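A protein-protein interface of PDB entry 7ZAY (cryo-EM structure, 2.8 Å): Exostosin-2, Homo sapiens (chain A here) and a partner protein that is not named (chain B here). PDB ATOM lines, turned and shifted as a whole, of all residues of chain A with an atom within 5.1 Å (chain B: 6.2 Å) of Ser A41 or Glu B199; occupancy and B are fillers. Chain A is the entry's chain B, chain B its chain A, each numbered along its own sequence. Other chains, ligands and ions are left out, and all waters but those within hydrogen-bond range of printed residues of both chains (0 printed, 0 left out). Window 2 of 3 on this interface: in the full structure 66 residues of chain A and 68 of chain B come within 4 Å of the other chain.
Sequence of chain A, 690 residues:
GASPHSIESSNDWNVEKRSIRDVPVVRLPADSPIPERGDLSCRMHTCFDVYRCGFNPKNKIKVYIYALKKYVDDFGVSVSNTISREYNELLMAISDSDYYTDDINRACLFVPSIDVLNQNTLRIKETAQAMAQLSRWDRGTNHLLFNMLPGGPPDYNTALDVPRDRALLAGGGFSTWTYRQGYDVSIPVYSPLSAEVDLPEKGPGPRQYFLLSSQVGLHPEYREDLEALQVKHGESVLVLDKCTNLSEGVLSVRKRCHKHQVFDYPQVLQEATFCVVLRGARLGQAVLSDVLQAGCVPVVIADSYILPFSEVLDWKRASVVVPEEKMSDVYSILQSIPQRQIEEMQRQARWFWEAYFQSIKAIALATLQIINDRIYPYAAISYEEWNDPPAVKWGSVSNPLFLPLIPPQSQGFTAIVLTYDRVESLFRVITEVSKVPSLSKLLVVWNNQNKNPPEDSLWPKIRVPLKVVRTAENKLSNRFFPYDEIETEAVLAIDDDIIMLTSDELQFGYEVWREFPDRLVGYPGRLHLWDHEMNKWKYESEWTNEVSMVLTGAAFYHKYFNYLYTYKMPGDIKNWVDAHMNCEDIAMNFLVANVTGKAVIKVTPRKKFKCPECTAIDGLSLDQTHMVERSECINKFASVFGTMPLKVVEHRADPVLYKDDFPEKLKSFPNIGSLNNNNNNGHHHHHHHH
The side-chain carboxylate (OE2) of Glu B199 lies within hydrogen-bond range of the side-chain hydroxyl (OG1) of Thr A46 (3.1 Å). A ring nitrogen (NE2) of His A45 sits close to the side-chain hydroxyl (OG1) of Thr B198 (2.2 Å).
The backbone carbonyl oxygen (O) of Gly B338 is in hydrogen-bond range of the side-chain hydroxyl (OG) of Ser B197 (3.1 Å). N of Thr B198 lies within hydrogen-bond range of OE1 of Glu B340, at 2.8 Å. O of Leu A40 is in hydrogen-bond range of NH1 of Arg A43 (3.3 Å). OG1 of Thr A46 sits at hydrogen-bond distance from N of Arg A43 (3.3 Å).
O of Ser A41 touches OE2 of Glu B199 (3.5 Å). Arg A43 touches Thr B198. Ser B197 touches His A45. CA of Gly B338 touches NE2 of His A45, 3.3 Å away.
Ser A41 touches one residue of chain B. Of the printed residues of chain B, His A45 touches Ser B197 (3.97 Å), Thr B198 (2.2 Å) and Gly B338 (3.3 Å). Ile B196 touches none of the printed residues of chain A. Of the printed residues of chain A, Thr B198 touches Arg A43 (3.3 Å) and His A45 (2.2 Å). Of chain A, only Ser A41 and Thr A46 come within 4 Å of Glu B199.
Of the 8 printed residues of chain A, 4 touch a printed residue of chain B. Printed residues of chain A that touch a printed residue of chain B: Ser A41, Arg A43, His A45 and Thr A46. Of the 8 printed residues of chain B, 4 touch a printed residue of chain A.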
ATOM      1  N   ASP A  39      -7.032  -2.945 -13.508  1.00  0.00           N
ATOM      2  CA  ASP A  39      -6.940  -2.222 -14.775  1.00  0.00           C
ATOM      3  C   ASP A  39      -7.950  -2.808 -15.752  1.00  0.00           C
ATOM      4  O   ASP A  39      -7.742  -3.888 -16.309  1.00  0.00           O
ATOM      5  CB  ASP A  39      -5.524  -2.306 -15.331  1.00  0.00           C
ATOM      6  CG  ASP A  39      -4.473  -1.926 -14.308  1.00  0.00           C
ATOM      7  OD1 ASP A  39      -4.802  -1.169 -13.371  1.00  0.00           O
ATOM      8  OD2 ASP A  39      -3.320  -2.386 -14.441  1.00  0.00           O
ATOM      9  N   LEU A  40      -9.054  -2.091 -15.968  1.00  0.00           N
ATOM     10  CA  LEU A  40     -10.102  -2.559 -16.867  1.00  0.00           C
ATOM     11  C   LEU A  40      -9.669  -2.568 -18.328  1.00  0.00           C
ATOM     12  O   LEU A  40     -10.379  -3.138 -19.163  1.00  0.00           O
ATOM     13  CB  LEU A  40     -11.353  -1.695 -16.698  1.00  0.00           C
ATOM     14  CG  LEU A  40     -12.692  -2.283 -17.145  1.00  0.00           C
ATOM     15  CD1 LEU A  40     -13.004  -3.553 -16.372  1.00  0.00           C
ATOM     16  CD2 LEU A  40     -13.804  -1.263 -16.974  1.00  0.00           C
ATOM     17  N   SER A  41      -8.532  -1.959 -18.655  1.00  0.00           N
ATOM     18  CA  SER A  41      -7.998  -1.983 -20.010  1.00  0.00           C
ATOM     19  C   SER A  41      -7.039  -3.142 -20.250  1.00  0.00           C
ATOM     20  O   SER A  41      -6.514  -3.270 -21.361  1.00  0.00           O
ATOM     21  CB  SER A  41      -7.290  -0.660 -20.319  1.00  0.00           C
ATOM     22  OG  SER A  41      -6.200  -0.448 -19.439  1.00  0.00           O
ATOM     23  N   CYS A  42      -6.795  -3.978 -19.244  1.00  0.00           N
ATOM     24  CA  CYS A  42      -5.890  -5.107 -19.408  1.00  0.00           C
ATOM     25  C   CYS A  42      -6.449  -6.118 -20.402  1.00  0.00           C
ATOM     26  O   CYS A  42      -7.646  -6.423 -20.399  1.00  0.00           O
ATOM     27  CB  CYS A  42      -5.636  -5.788 -18.064  1.00  0.00           C
ATOM     28  SG  CYS A  42      -4.122  -5.255 -17.239  1.00  0.00           S
ATOM     29  N   ARG A  43      -5.569  -6.639 -21.253  1.00  0.00           N
ATOM     30  CA  ARG A  43      -5.929  -7.641 -22.244  1.00  0.00           C
ATOM     31  C   ARG A  43      -4.834  -8.697 -22.299  1.00  0.00           C
ATOM     32  O   ARG A  43      -3.770  -8.554 -21.691  1.00  0.00           O
ATOM     33  CB  ARG A  43      -6.149  -7.015 -23.626  1.00  0.00           C
ATOM     34  CG  ARG A  43      -7.428  -6.201 -23.745  1.00  0.00           C
ATOM     35  CD  ARG A  43      -8.650  -7.041 -23.414  1.00  0.00           C
ATOM     36  NE  ARG A  43      -9.894  -6.355 -23.746  1.00  0.00           N
ATOM     37  CZ  ARG A  43     -10.516  -5.501 -22.946  1.00  0.00           C
ATOM     38  NH1 ARG A  43     -10.025  -5.183 -21.758  1.00  0.00           N
ATOM     39  NH2 ARG A  43     -11.656  -4.948 -23.347  1.00  0.00           N
ATOM     40  N   HIS A  45      -2.820  -9.418 -24.532  1.00  0.00           N
ATOM     41  CA  HIS A  45      -1.614  -9.016 -25.238  1.00  0.00           C
ATOM     42  C   HIS A  45      -0.868  -7.870 -24.573  1.00  0.00           C
ATOM     43  O   HIS A  45       0.318  -7.683 -24.858  1.00  0.00           O
ATOM     44  CB  HIS A  45      -1.955  -8.613 -26.680  1.00  0.00           C
ATOM     45  CG  HIS A  45      -3.051  -7.598 -26.775  1.00  0.00           C
ATOM     46  ND1 HIS A  45      -2.808  -6.259 -26.991  1.00  0.00           N
ATOM     47  CD2 HIS A  45      -4.394  -7.724 -26.669  1.00  0.00           C
ATOM     48  CE1 HIS A  45      -3.955  -5.605 -27.022  1.00  0.00           C
ATOM     49  NE2 HIS A  45      -4.933  -6.471 -26.830  1.00  0.00           N
ATOM     50  N   THR A  46      -1.527  -7.106 -23.700  1.00  0.00           N
ATOM     51  CA  THR A  46      -0.893  -5.985 -23.022  1.00  0.00           C
ATOM     52  C   THR A  46      -0.595  -6.243 -21.553  1.00  0.00           C
ATOM     53  O   THR A  46       0.248  -5.545 -20.983  1.00  0.00           O
ATOM     54  CB  THR A  46      -1.767  -4.727 -23.131  1.00  0.00           C
ATOM     55  OG1 THR A  46      -3.099  -5.028 -22.696  1.00  0.00           O
ATOM     56  CG2 THR A  46      -1.805  -4.226 -24.566  1.00  0.00           C
ATOM     57  N   ARG A 180     -13.471  -7.536 -18.752  1.00  0.00           N
ATOM     58  CA  ARG A 180     -12.414  -7.487 -19.750  1.00  0.00           C
ATOM     59  C   ARG A 180     -12.582  -8.639 -20.733  1.00  0.00           C
ATOM     60  O   ARG A 180     -12.115  -9.755 -20.477  1.00  0.00           O
ATOM     61  CB  ARG A 180     -11.049  -7.536 -19.064  1.00  0.00           C
ATOM     62  CG  ARG A 180     -10.753  -6.298 -18.235  1.00  0.00           C
ATOM     63  CD  ARG A 180      -9.525  -6.475 -17.360  1.00  0.00           C
ATOM     64  NE  ARG A 180      -9.730  -7.498 -16.342  1.00  0.00           N
ATOM     65  CZ  ARG A 180      -8.828  -7.840 -15.432  1.00  0.00           C
ATOM     66  NH1 ARG A 180      -7.648  -7.246 -15.371  1.00  0.00           N
ATOM     67  NH2 ARG A 180      -9.120  -8.799 -14.558  1.00  0.00           N
ATOM     68  N   ILE B 196      -8.993  -2.292 -35.400  1.00  0.00           N
ATOM     69  CA  ILE B 196      -9.292  -1.801 -34.059  1.00  0.00           C
ATOM     70  C   ILE B 196      -8.613  -2.709 -33.043  1.00  0.00           C
ATOM     71  O   ILE B 196      -8.576  -3.932 -33.214  1.00  0.00           O
ATOM     72  CB  ILE B 196     -10.815  -1.736 -33.834  1.00  0.00           C
ATOM     73  CG1 ILE B 196     -11.150  -1.506 -32.360  1.00  0.00           C
ATOM     74  CG2 ILE B 196     -11.485  -3.004 -34.340  1.00  0.00           C
ATOM     75  CD1 ILE B 196     -10.722  -0.158 -31.839  1.00  0.00           C
ATOM     76  N   SER B 197      -8.047  -2.113 -31.997  1.00  0.00           N
ATOM     77  CA  SER B 197      -7.374  -2.865 -30.946  1.00  0.00           C
ATOM     78  C   SER B 197      -8.343  -3.200 -29.816  1.00  0.00           C
ATOM     79  O   SER B 197      -9.327  -2.495 -29.586  1.00  0.00           O
ATOM     80  CB  SER B 197      -6.185  -2.079 -30.395  1.00  0.00           C
ATOM     81  OG  SER B 197      -5.472  -2.844 -29.440  1.00  0.00           O
ATOM     82  N   THR B 198      -8.049  -4.299 -29.111  1.00  0.00           N
ATOM     83  CA  THR B 198      -8.940  -4.767 -28.052  1.00  0.00           C
ATOM     84  C   THR B 198      -9.070  -3.751 -26.925  1.00  0.00           C
ATOM     85  O   THR B 198     -10.128  -3.663 -26.291  1.00  0.00           O
ATOM     86  CB  THR B 198      -8.446  -6.101 -27.484  1.00  0.00           C
ATOM     87  OG1 THR B 198      -7.102  -5.951 -27.013  1.00  0.00           O
ATOM     88  CG2 THR B 198      -8.497  -7.198 -28.529  1.00  0.00           C
ATOM     89  N   GLU B 199      -8.011  -2.985 -26.655  1.00  0.00           N
ATOM     90  CA  GLU B 199      -8.081  -1.973 -25.604  1.00  0.00           C
ATOM     91  C   GLU B 199      -9.129  -0.917 -25.924  1.00  0.00           C
ATOM     92  O   GLU B 199      -9.872  -0.479 -25.037  1.00  0.00           O
ATOM     93  CB  GLU B 199      -6.711  -1.328 -25.401  1.00  0.00           C
ATOM     94  CG  GLU B 199      -5.711  -2.214 -24.681  1.00  0.00           C
ATOM     95  CD  GLU B 199      -4.607  -1.421 -24.010  1.00  0.00           C
ATOM     96  OE1 GLU B 199      -4.527  -0.197 -24.242  1.00  0.00           O
ATOM     97  OE2 GLU B 199      -3.820  -2.020 -23.247  1.00  0.00           O
ATOM     98  N   ASN B 200      -9.206  -0.496 -27.183  1.00  0.00           N
ATOM     99  CA  ASN B 200     -10.138   0.539 -27.606  1.00  0.00           C
ATOM    100  C   ASN B 200     -11.457  -0.028 -28.110  1.00  0.00           C
ATOM    101  O   ASN B 200     -12.330   0.743 -28.520  1.00  0.00           O
ATOM    102  CB  ASN B 200      -9.499   1.405 -28.695  1.00  0.00           C
ATOM    103  CG  ASN B 200      -8.039   1.700 -28.418  1.00  0.00           C
ATOM    104  OD1 ASN B 200      -7.631   1.847 -27.266  1.00  0.00           O
ATOM    105  ND2 ASN B 200      -7.241   1.780 -29.475  1.00  0.00           N
ATOM    106  N   PHE B 201     -11.619  -1.347 -28.092  1.00  0.00           N
ATOM    107  CA  PHE B 201     -12.825  -1.975 -28.606  1.00  0.00           C
ATOM    108  C   PHE B 201     -13.952  -1.904 -27.585  1.00  0.00           C
ATOM    109  O   PHE B 201     -13.728  -1.938 -26.372  1.00  0.00           O
ATOM    110  CB  PHE B 201     -12.553  -3.432 -28.972  1.00  0.00           C
ATOM    111  CG  PHE B 201     -13.609  -4.051 -29.842  1.00  0.00           C
ATOM    112  CD1 PHE B 201     -13.673  -3.756 -31.193  1.00  0.00           C
ATOM    113  CD2 PHE B 201     -14.530  -4.938 -29.312  1.00  0.00           C
ATOM    114  CE1 PHE B 201     -14.639  -4.326 -31.996  1.00  0.00           C
ATOM    115  CE2 PHE B 201     -15.499  -5.511 -30.110  1.00  0.00           C
ATOM    116  CZ  PHE B 201     -15.553  -5.205 -31.453  1.00  0.00           C
ATOM    117  N   GLY B 338      -3.251  -8.094 -30.389  1.00  0.00           N
ATOM    118  CA  GLY B 338      -4.346  -7.218 -30.019  1.00  0.00           C
ATOM    119  C   GLY B 338      -5.109  -6.620 -31.179  1.00  0.00           C
ATOM    120  O   GLY B 338      -5.427  -5.425 -31.156  1.00  0.00           O
ATOM    121  N   GLU B 340      -8.676  -7.244 -33.250  1.00  0.00           N
ATOM    122  CA  GLU B 340      -9.920  -7.978 -33.429  1.00  0.00           C
ATOM    123  C   GLU B 340     -10.053  -8.365 -34.892  1.00  0.00           C
ATOM    124  O   GLU B 340     -10.161  -7.494 -35.763  1.00  0.00           O
ATOM    125  CB  GLU B 340     -11.119  -7.143 -32.991  1.00  0.00           C
ATOM    126  CG  GLU B 340     -11.104  -6.735 -31.536  1.00  0.00           C
ATOM    127  CD  GLU B 340     -10.155  -5.590 -31.280  1.00  0.00           C
ATOM    128  OE1 GLU B 340      -8.930  -5.827 -31.256  1.00  0.00           O
ATOM    129  OE2 GLU B 340     -10.632  -4.449 -31.133  1.00  0.00           O
